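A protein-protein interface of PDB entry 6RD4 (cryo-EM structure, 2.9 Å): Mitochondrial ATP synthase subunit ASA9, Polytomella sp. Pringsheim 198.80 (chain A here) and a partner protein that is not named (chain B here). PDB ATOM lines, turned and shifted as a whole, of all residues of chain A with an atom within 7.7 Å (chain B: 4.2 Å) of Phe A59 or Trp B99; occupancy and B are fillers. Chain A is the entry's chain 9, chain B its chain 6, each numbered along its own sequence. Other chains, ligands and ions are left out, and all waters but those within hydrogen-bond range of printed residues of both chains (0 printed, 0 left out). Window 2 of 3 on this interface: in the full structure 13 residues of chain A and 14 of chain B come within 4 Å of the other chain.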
ATOM      1  N   LEU A  52      25.457 -22.406   5.504  1.00  0.00           N
ATOM      2  CA  LEU A  52      24.116 -21.942   5.156  1.00  0.00           C
ATOM      3  C   LEU A  52      23.710 -20.723   5.963  1.00  0.00           C
ATOM      4  O   LEU A  52      23.004 -19.856   5.448  1.00  0.00           O
ATOM      5  CB  LEU A  52      23.089 -23.053   5.366  1.00  0.00           C
ATOM      6  CG  LEU A  52      22.614 -23.904   4.193  1.00  0.00           C
ATOM      7  CD1 LEU A  52      21.819 -23.048   3.255  1.00  0.00           C
ATOM      8  CD2 LEU A  52      23.758 -24.549   3.459  1.00  0.00           C
ATOM      9  N   LEU A  53      24.159 -20.629   7.208  1.00  0.00           N
ATOM     10  CA  LEU A  53      23.869 -19.445   8.000  1.00  0.00           C
ATOM     11  C   LEU A  53      24.690 -18.258   7.525  1.00  0.00           C
ATOM     12  O   LEU A  53      24.153 -17.170   7.310  1.00  0.00           O
ATOM     13  CB  LEU A  53      24.143 -19.722   9.471  1.00  0.00           C
ATOM     14  CG  LEU A  53      23.055 -20.477  10.212  1.00  0.00           C
ATOM     15  CD1 LEU A  53      23.399 -20.601  11.663  1.00  0.00           C
ATOM     16  CD2 LEU A  53      21.762 -19.756  10.060  1.00  0.00           C
ATOM     17  N   ALA A  54      25.988 -18.458   7.325  1.00  0.00           N
ATOM     18  CA  ALA A  54      26.872 -17.350   7.016  1.00  0.00           C
ATOM     19  C   ALA A  54      26.698 -16.829   5.602  1.00  0.00           C
ATOM     20  O   ALA A  54      27.024 -15.669   5.350  1.00  0.00           O
ATOM     21  CB  ALA A  54      28.321 -17.765   7.225  1.00  0.00           C
ATOM     22  N   ALA A  55      26.190 -17.640   4.677  1.00  0.00           N
ATOM     23  CA  ALA A  55      26.031 -17.180   3.305  1.00  0.00           C
ATOM     24  C   ALA A  55      24.932 -16.144   3.171  1.00  0.00           C
ATOM     25  O   ALA A  55      24.901 -15.419   2.177  1.00  0.00           O
ATOM     26  CB  ALA A  55      25.756 -18.351   2.365  1.00  0.00           C
ATOM     27  N   ASN A  56      24.019 -16.079   4.126  1.00  0.00           N
ATOM     28  CA  ASN A  56      23.134 -14.927   4.280  1.00  0.00           C
ATOM     29  C   ASN A  56      22.975 -14.718   5.777  1.00  0.00           C
ATOM     30  O   ASN A  56      22.056 -15.258   6.384  1.00  0.00           O
ATOM     31  CB  ASN A  56      21.802 -15.152   3.587  1.00  0.00           C
ATOM     32  CG  ASN A  56      21.314 -16.568   3.714  1.00  0.00           C
ATOM     33  OD1 ASN A  56      21.939 -17.395   4.360  1.00  0.00           O
ATOM     34  ND2 ASN A  56      20.200 -16.862   3.081  1.00  0.00           N
ATOM     35  N   PHE A  57      23.877 -13.943   6.371  1.00  0.00           N
ATOM     36  CA  PHE A  57      23.795 -13.810   7.820  1.00  0.00           C
ATOM     37  C   PHE A  57      22.780 -12.782   8.312  1.00  0.00           C
ATOM     38  O   PHE A  57      22.031 -13.117   9.239  1.00  0.00           O
ATOM     39  CB  PHE A  57      25.143 -13.493   8.463  1.00  0.00           C
ATOM     40  CG  PHE A  57      25.009 -12.995   9.871  1.00  0.00           C
ATOM     41  CD1 PHE A  57      25.270 -11.673  10.186  1.00  0.00           C
ATOM     42  CD2 PHE A  57      24.583 -13.845  10.881  1.00  0.00           C
ATOM     43  CE1 PHE A  57      25.113 -11.224  11.466  1.00  0.00           C
ATOM     44  CE2 PHE A  57      24.425 -13.389  12.154  1.00  0.00           C
ATOM     45  CZ  PHE A  57      24.695 -12.085  12.449  1.00  0.00           C
ATOM     46  N   PRO A  58      22.735 -11.508   7.821  1.00  0.00           N
ATOM     47  CA  PRO A  58      21.749 -10.597   8.408  1.00  0.00           C
ATOM     48  C   PRO A  58      20.345 -11.002   8.011  1.00  0.00           C
ATOM     49  O   PRO A  58      19.824 -10.538   7.002  1.00  0.00           O
ATOM     50  CB  PRO A  58      22.130  -9.231   7.830  1.00  0.00           C
ATOM     51  CG  PRO A  58      23.475  -9.398   7.313  1.00  0.00           C
ATOM     52  CD  PRO A  58      23.524 -10.776   6.813  1.00  0.00           C
ATOM     53  N   PHE A  59      19.766 -11.941   8.751  1.00  0.00           N
ATOM     54  CA  PHE A  59      18.396 -12.335   8.510  1.00  0.00           C
ATOM     55  C   PHE A  59      17.711 -12.533   9.845  1.00  0.00           C
ATOM     56  O   PHE A  59      18.326 -12.944  10.825  1.00  0.00           O
ATOM     57  CB  PHE A  59      18.286 -13.591   7.622  1.00  0.00           C
ATOM     58  CG  PHE A  59      18.575 -14.892   8.323  1.00  0.00           C
ATOM     59  CD1 PHE A  59      19.863 -15.296   8.538  1.00  0.00           C
ATOM     60  CD2 PHE A  59      17.557 -15.718   8.734  1.00  0.00           C
ATOM     61  CE1 PHE A  59      20.145 -16.471   9.149  1.00  0.00           C
ATOM     62  CE2 PHE A  59      17.837 -16.893   9.362  1.00  0.00           C
ATOM     63  CZ  PHE A  59      19.136 -17.262   9.569  1.00  0.00           C
ATOM     64  N   ASN A  60      16.450 -12.180   9.877  1.00  0.00           N
ATOM     65  CA  ASN A  60      15.628 -12.457  11.029  1.00  0.00           C
ATOM     66  C   ASN A  60      15.276 -13.934  11.018  1.00  0.00           C
ATOM     67  O   ASN A  60      14.741 -14.419  10.018  1.00  0.00           O
ATOM     68  CB  ASN A  60      14.383 -11.608  10.981  1.00  0.00           C
ATOM     69  CG  ASN A  60      13.764 -11.433  12.312  1.00  0.00           C
ATOM     70  OD1 ASN A  60      14.416 -11.576  13.325  1.00  0.00           O
ATOM     71  ND2 ASN A  60      12.498 -11.097  12.330  1.00  0.00           N
ATOM     72  N   PRO A  61      15.574 -14.681  12.069  1.00  0.00           N
ATOM     73  CA  PRO A  61      15.458 -16.120  12.007  1.00  0.00           C
ATOM     74  C   PRO A  61      14.014 -16.578  12.031  1.00  0.00           C
ATOM     75  O   PRO A  61      13.223 -16.130  12.872  1.00  0.00           O
ATOM     76  CB  PRO A  61      16.198 -16.577  13.262  1.00  0.00           C
ATOM     77  CG  PRO A  61      16.151 -15.458  14.150  1.00  0.00           C
ATOM     78  CD  PRO A  61      16.248 -14.257  13.301  1.00  0.00           C
ATOM     79  N   PRO A  62      13.638 -17.478  11.121  1.00  0.00           N
ATOM     80  CA  PRO A  62      12.324 -18.114  11.222  1.00  0.00           C
ATOM     81  C   PRO A  62      12.221 -19.034  12.408  1.00  0.00           C
ATOM     82  O   PRO A  62      11.155 -19.134  13.023  1.00  0.00           O
ATOM     83  CB  PRO A  62      12.220 -18.902   9.918  1.00  0.00           C
ATOM     84  CG  PRO A  62      13.326 -18.448   9.079  1.00  0.00           C
ATOM     85  CD  PRO A  62      14.395 -18.000   9.984  1.00  0.00           C
ATOM     86  N   PHE A  63      13.303 -19.716  12.731  1.00  0.00           N
ATOM     87  CA  PHE A  63      13.336 -20.615  13.857  1.00  0.00           C
ATOM     88  C   PHE A  63      13.327 -19.827  15.158  1.00  0.00           C
ATOM     89  O   PHE A  63      13.763 -18.678  15.193  1.00  0.00           O
ATOM     90  CB  PHE A  63      14.577 -21.487  13.792  1.00  0.00           C
ATOM     91  CG  PHE A  63      15.854 -20.747  13.538  1.00  0.00           C
ATOM     92  CD1 PHE A  63      16.339 -20.596  12.259  1.00  0.00           C
ATOM     93  CD2 PHE A  63      16.608 -20.274  14.588  1.00  0.00           C
ATOM     94  CE1 PHE A  63      17.517 -19.951  12.035  1.00  0.00           C
ATOM     95  CE2 PHE A  63      17.786 -19.632  14.362  1.00  0.00           C
ATOM     96  CZ  PHE A  63      18.241 -19.475  13.085  1.00  0.00           C
ATOM     97  N   PRO A  70      22.871 -12.496  17.979  1.00  0.00           N
ATOM     98  CA  PRO A  70      24.116 -12.912  17.318  1.00  0.00           C
ATOM     99  C   PRO A  70      25.386 -12.183  17.725  1.00  0.00           C
ATOM    100  O   PRO A  70      26.397 -12.790  18.081  1.00  0.00           O
ATOM    101  CB  PRO A  70      23.817 -12.651  15.842  1.00  0.00           C
ATOM    102  CG  PRO A  70      22.370 -12.603  15.741  1.00  0.00           C
ATOM    103  CD  PRO A  70      21.884 -12.025  17.000  1.00  0.00           C
ATOM    104  N   TRP A  73      23.810  -6.740  17.834  1.00  0.00           N
ATOM    105  CA  TRP A  73      22.523  -6.339  17.286  1.00  0.00           C
ATOM    106  C   TRP A  73      21.497  -6.087  18.385  1.00  0.00           C
ATOM    107  O   TRP A  73      21.077  -4.944  18.574  1.00  0.00           O
ATOM    108  CB  TRP A  73      22.028  -7.412  16.301  1.00  0.00           C
ATOM    109  CG  TRP A  73      23.017  -7.777  15.211  1.00  0.00           C
ATOM    110  CD1 TRP A  73      24.104  -8.593  15.316  1.00  0.00           C
ATOM    111  CD2 TRP A  73      22.997  -7.319  13.857  1.00  0.00           C
ATOM    112  NE1 TRP A  73      24.760  -8.668  14.116  1.00  0.00           N
ATOM    113  CE2 TRP A  73      24.097  -7.897  13.204  1.00  0.00           C
ATOM    114  CE3 TRP A  73      22.156  -6.476  13.139  1.00  0.00           C
ATOM    115  CZ2 TRP A  73      24.375  -7.654  11.874  1.00  0.00           C
ATOM    116  CZ3 TRP A  73      22.431  -6.243  11.820  1.00  0.00           C
ATOM    117  CH2 TRP A  73      23.532  -6.827  11.198  1.00  0.00           C
ATOM    118  N   TRP A  77      16.495  -5.283  13.998  1.00  0.00           N
ATOM    119  CA  TRP A  77      15.540  -6.118  13.292  1.00  0.00           C
ATOM    120  C   TRP A  77      15.957  -7.575  13.265  1.00  0.00           C
ATOM    121  O   TRP A  77      15.103  -8.445  13.094  1.00  0.00           O
ATOM    122  CB  TRP A  77      15.381  -5.612  11.874  1.00  0.00           C
ATOM    123  CG  TRP A  77      16.646  -5.618  11.110  1.00  0.00           C
ATOM    124  CD1 TRP A  77      17.640  -4.699  11.160  1.00  0.00           C
ATOM    125  CD2 TRP A  77      17.050  -6.588  10.151  1.00  0.00           C
ATOM    126  NE1 TRP A  77      18.647  -5.039  10.302  1.00  0.00           N
ATOM    127  CE2 TRP A  77      18.302  -6.198   9.664  1.00  0.00           C
ATOM    128  CE3 TRP A  77      16.469  -7.753   9.655  1.00  0.00           C
ATOM    129  CZ2 TRP A  77      18.983  -6.929   8.714  1.00  0.00           C
ATOM    130  CZ3 TRP A  77      17.143  -8.465   8.715  1.00  0.00           C
ATOM    131  CH2 TRP A  77      18.384  -8.053   8.249  1.00  0.00           C
ATOM    132  N   VAL A  78      17.250  -7.856  13.427  1.00  0.00           N
ATOM    133  CA  VAL A  78      17.744  -9.222  13.375  1.00  0.00           C
ATOM    134  C   VAL A  78      17.278 -10.012  14.584  1.00  0.00           C
ATOM    135  O   VAL A  78      16.987 -11.205  14.483  1.00  0.00           O
ATOM    136  CB  VAL A  78      19.275  -9.189  13.237  1.00  0.00           C
ATOM    137  CG1 VAL A  78      19.909 -10.536  13.465  1.00  0.00           C
ATOM    138  CG2 VAL A  78      19.638  -8.703  11.874  1.00  0.00           C
ATOM    139  N   CYS A  79      17.133  -9.369  15.730  1.00  0.00           N
ATOM    140  CA  CYS A  79      16.758 -10.086  16.934  1.00  0.00           C
ATOM    141  C   CYS A  79      15.305  -9.888  17.320  1.00  0.00           C
ATOM    142  O   CYS A  79      14.889 -10.374  18.373  1.00  0.00           O
ATOM    143  CB  CYS A  79      17.649  -9.662  18.095  1.00  0.00           C
ATOM    144  SG  CYS A  79      19.366  -9.505  17.644  1.00  0.00           S
ATOM    145  N   LYS A  83       7.518 -10.356  13.845  1.00  0.00           N
ATOM    146  CA  LYS A  83       8.011 -10.350  12.476  1.00  0.00           C
ATOM    147  C   LYS A  83       7.498  -9.166  11.675  1.00  0.00           C
ATOM    148  O   LYS A  83       8.236  -8.632  10.846  1.00  0.00           O
ATOM    149  CB  LYS A  83       7.649 -11.663  11.801  1.00  0.00           C
ATOM    150  CG  LYS A  83       8.175 -12.861  12.552  1.00  0.00           C
ATOM    151  CD  LYS A  83       9.667 -12.741  12.752  1.00  0.00           C
ATOM    152  CE  LYS A  83      10.198 -13.743  13.741  1.00  0.00           C
ATOM    153  NZ  LYS A  83      11.614 -13.460  14.033  1.00  0.00           N
ATOM    154  N   TYR A  90      13.726  -3.537   9.305  1.00  0.00           N
ATOM    155  CA  TYR A  90      14.672  -3.901   8.255  1.00  0.00           C
ATOM    156  C   TYR A  90      14.609  -2.912   7.104  1.00  0.00           C
ATOM    157  O   TYR A  90      15.636  -2.582   6.503  1.00  0.00           O
ATOM    158  CB  TYR A  90      14.393  -5.322   7.756  1.00  0.00           C
ATOM    159  CG  TYR A  90      15.036  -5.647   6.429  1.00  0.00           C
ATOM    160  CD1 TYR A  90      16.403  -5.824   6.331  1.00  0.00           C
ATOM    161  CD2 TYR A  90      14.277  -5.772   5.278  1.00  0.00           C
ATOM    162  CE1 TYR A  90      16.994  -6.110   5.130  1.00  0.00           C
ATOM    163  CE2 TYR A  90      14.863  -6.052   4.075  1.00  0.00           C
ATOM    164  CZ  TYR A  90      16.220  -6.219   4.009  1.00  0.00           C
ATOM    165  OH  TYR A  90      16.809  -6.501   2.806  1.00  0.00           O
ATOM    166  N   GLN B  93      11.785 -24.337  -1.706  1.00  0.00           N
ATOM    167  CA  GLN B  93      12.270 -24.520  -0.348  1.00  0.00           C
ATOM    168  C   GLN B  93      12.831 -23.245   0.216  1.00  0.00           C
ATOM    169  O   GLN B  93      12.844 -23.073   1.434  1.00  0.00           O
ATOM    170  CB  GLN B  93      13.371 -25.563  -0.290  1.00  0.00           C
ATOM    171  CG  GLN B  93      12.946 -26.949   0.026  1.00  0.00           C
ATOM    172  CD  GLN B  93      14.127 -27.841   0.181  1.00  0.00           C
ATOM    173  OE1 GLN B  93      15.244 -27.452  -0.117  1.00  0.00           O
ATOM    174  NE2 GLN B  93      13.896 -29.048   0.647  1.00  0.00           N
ATOM    175  N   SER B  94      13.322 -22.363  -0.634  1.00  0.00           N
ATOM    176  CA  SER B  94      13.960 -21.143  -0.188  1.00  0.00           C
ATOM    177  C   SER B  94      12.975 -20.032   0.085  1.00  0.00           C
ATOM    178  O   SER B  94      13.394 -18.964   0.516  1.00  0.00           O
ATOM    179  CB  SER B  94      14.951 -20.683  -1.230  1.00  0.00           C
ATOM    180  OG  SER B  94      14.263 -20.331  -2.407  1.00  0.00           O
ATOM    181  N   ALA B  96       9.901 -20.789   1.954  1.00  0.00           N
ATOM    182  CA  ALA B  96       8.926 -21.695   2.536  1.00  0.00           C
ATOM    183  C   ALA B  96       8.512 -21.320   3.945  1.00  0.00           C
ATOM    184  O   ALA B  96       7.852 -22.130   4.603  1.00  0.00           O
ATOM    185  CB  ALA B  96       9.476 -23.116   2.539  1.00  0.00           C
ATOM    186  N   HIS B  97       8.932 -20.150   4.429  1.00  0.00           N
ATOM    187  CA  HIS B  97       8.753 -19.571   5.765  1.00  0.00           C
ATOM    188  C   HIS B  97       9.596 -20.262   6.827  1.00  0.00           C
ATOM    189  O   HIS B  97       9.855 -19.693   7.884  1.00  0.00           O
ATOM    190  CB  HIS B  97       7.280 -19.548   6.205  1.00  0.00           C
ATOM    191  CG  HIS B  97       7.050 -18.808   7.483  1.00  0.00           C
ATOM    192  ND1 HIS B  97       7.007 -17.435   7.548  1.00  0.00           N
ATOM    193  CD2 HIS B  97       6.925 -19.251   8.754  1.00  0.00           C
ATOM    194  CE1 HIS B  97       6.831 -17.064   8.801  1.00  0.00           C
ATOM    195  NE2 HIS B  97       6.781 -18.147   9.553  1.00  0.00           N
ATOM    196  N   GLU B  98      10.122 -21.431   6.533  1.00  0.00           N
ATOM    197  CA  GLU B  98      11.105 -22.097   7.363  1.00  0.00           C
ATOM    198  C   GLU B  98      12.287 -22.432   6.503  1.00  0.00           C
ATOM    199  O   GLU B  98      12.848 -23.521   6.567  1.00  0.00           O
ATOM    200  CB  GLU B  98      10.526 -23.346   8.000  1.00  0.00           C
ATOM    201  CG  GLU B  98       9.336 -23.100   8.892  1.00  0.00           C
ATOM    202  CD  GLU B  98       9.724 -22.834  10.329  1.00  0.00           C
ATOM    203  OE1 GLU B  98      10.915 -22.987  10.662  1.00  0.00           O
ATOM    204  OE2 GLU B  98       8.840 -22.468  11.128  1.00  0.00           O
ATOM    205  N   TRP B  99      12.664 -21.461   5.675  1.00  0.00           N
ATOM    206  CA  TRP B  99      13.512 -21.705   4.518  1.00  0.00           C
ATOM    207  C   TRP B  99      14.908 -22.121   4.928  1.00  0.00           C
ATOM    208  O   TRP B  99      15.538 -22.929   4.253  1.00  0.00           O
ATOM    209  CB  TRP B  99      13.569 -20.452   3.648  1.00  0.00           C
ATOM    210  CG  TRP B  99      14.027 -19.265   4.388  1.00  0.00           C
ATOM    211  CD1 TRP B  99      13.268 -18.418   5.106  1.00  0.00           C
ATOM    212  CD2 TRP B  99      15.366 -18.804   4.509  1.00  0.00           C
ATOM    213  NE1 TRP B  99      14.044 -17.452   5.675  1.00  0.00           N
ATOM    214  CE2 TRP B  99      15.343 -17.675   5.321  1.00  0.00           C
ATOM    215  CE3 TRP B  99      16.587 -19.248   4.018  1.00  0.00           C
ATOM    216  CZ2 TRP B  99      16.480 -16.984   5.643  1.00  0.00           C
ATOM    217  CZ3 TRP B  99      17.705 -18.564   4.343  1.00  0.00           C
ATOM    218  CH2 TRP B  99      17.652 -17.444   5.143  1.00  0.00           C
ATOM    219  N   ILE B 100      15.411 -21.585   6.034  1.00  0.00           N
ATOM    220  CA  ILE B 100      16.738 -21.959   6.475  1.00  0.00           C
ATOM    221  C   ILE B 100      16.692 -23.303   7.170  1.00  0.00           C
ATOM    222  O   ILE B 100      17.685 -24.029   7.176  1.00  0.00           O
ATOM    223  CB  ILE B 100      17.326 -20.829   7.342  1.00  0.00           C
ATOM    224  CG1 ILE B 100      18.806 -21.040   7.629  1.00  0.00           C
ATOM    225  CG2 ILE B 100      16.565 -20.665   8.607  1.00  0.00           C
ATOM    226  CD1 ILE B 100      19.642 -21.133   6.412  1.00  0.00           C
ATOM    227  N   VAL B 101      15.545 -23.695   7.705  1.00  0.00           N
ATOM    228  CA  VAL B 101      15.436 -25.030   8.264  1.00  0.00           C
ATOM    229  C   VAL B 101      15.242 -26.047   7.149  1.00  0.00           C
ATOM    230  O   VAL B 101      15.761 -27.161   7.220  1.00  0.00           O
ATOM    231  CB  VAL B 101      14.308 -25.062   9.301  1.00  0.00           C
ATOM    232  CG1 VAL B 101      14.230 -26.398   9.958  1.00  0.00           C
ATOM    233  CG2 VAL B 101      14.539 -23.995  10.330  1.00  0.00           C
ATOM    234  N   ASP B 102      14.527 -25.670   6.088  1.00  0.00           N
ATOM    235  CA  ASP B 102      14.355 -26.561   4.947  1.00  0.00           C
ATOM    236  C   ASP B 102      15.664 -26.778   4.217  1.00  0.00           C
ATOM    237  O   ASP B 102      15.974 -27.899   3.823  1.00  0.00           O
ATOM    238  CB  ASP B 102      13.333 -26.005   3.966  1.00  0.00           C
ATOM    239  CG  ASP B 102      11.938 -26.029   4.504  1.00  0.00           C
ATOM    240  OD1 ASP B 102      11.790 -26.216   5.713  1.00  0.00           O
ATOM    241  OD2 ASP B 102      10.988 -25.859   3.720  1.00  0.00           O
ATOM    242  N   LEU B 103      16.447 -25.724   4.029  1.00  0.00           N
ATOM    243  CA  LEU B 103      17.709 -25.869   3.328  1.00  0.00           C
ATOM    244  C   LEU B 103      18.777 -26.514   4.188  1.00  0.00           C
ATOM    245  O   LEU B 103      19.755 -27.023   3.647  1.00  0.00           O
ATOM    246  CB  LEU B 103      18.192 -24.516   2.838  1.00  0.00           C
ATOM    247  CG  LEU B 103      17.366 -23.904   1.720  1.00  0.00           C
ATOM    248  CD1 LEU B 103      17.759 -22.479   1.612  1.00  0.00           C
ATOM    249  CD2 LEU B 103      17.558 -24.601   0.413  1.00  0.00           C
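The side-chain amide oxygen (OD1) of Asn A56 lies close to the backbone carbonyl oxygen (O) of Leu A52 (2.9 Å).
Leu A52 touches Ile B100 (O to CD1, 3.7 Å).
CD1 of Leu A52 touches CB of Leu B103 (3.9 Å).
Asn A56 touches Trp B99 (ND2 to CZ3, 3.3 Å).
Trp B99 touches Phe A59 (CZ2 to CD2, 3.5 Å).
His B97 touches Pro A62 (O to CB, 3.2 Å).
Pro A62 touches Trp B99.
Ile B100 touches Pro A62.
Ile B100 touches Phe A63.
Phe A59 touches just one residue of chain B: Trp B99.
Of the printed residues of chain B, Pro A62 touches His B97 (3.2 Å), Trp B99 (3.6 Å) and Ile B100 (3.7 Å).
Of the printed residues of chain B, Phe A63 touches Ile B100.
Trp B99 touches just these residues of chain A: Asn A56, Phe A59 and Pro A62.
Of the printed residues of chain A, Leu B103 touches Leu A52 (3.9 Å).
The nearest residue of chain B that does not touch Phe A59 is Ile B100 (4.1 Å).
The nearest printed residue of chain B that does not touch Leu A52 is Trp B99 (5.6 Å).
Printed residues of chain B that touch a printed residue of chain A: His B97, Trp B99, Ile B100 and Leu B103.
Hydrophobic or aromatic side chains of chain B within 4 Å of the printed part of chain A: Trp B99, Ile B100 and Leu B103.
Of the 19 printed residues of chain A, 5 touch a printed residue of chain B.
Among the printed residues, no Asp or Glu carboxylate lies within 4 Å of a Lys or Arg side-chain nitrogen of the other chain.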
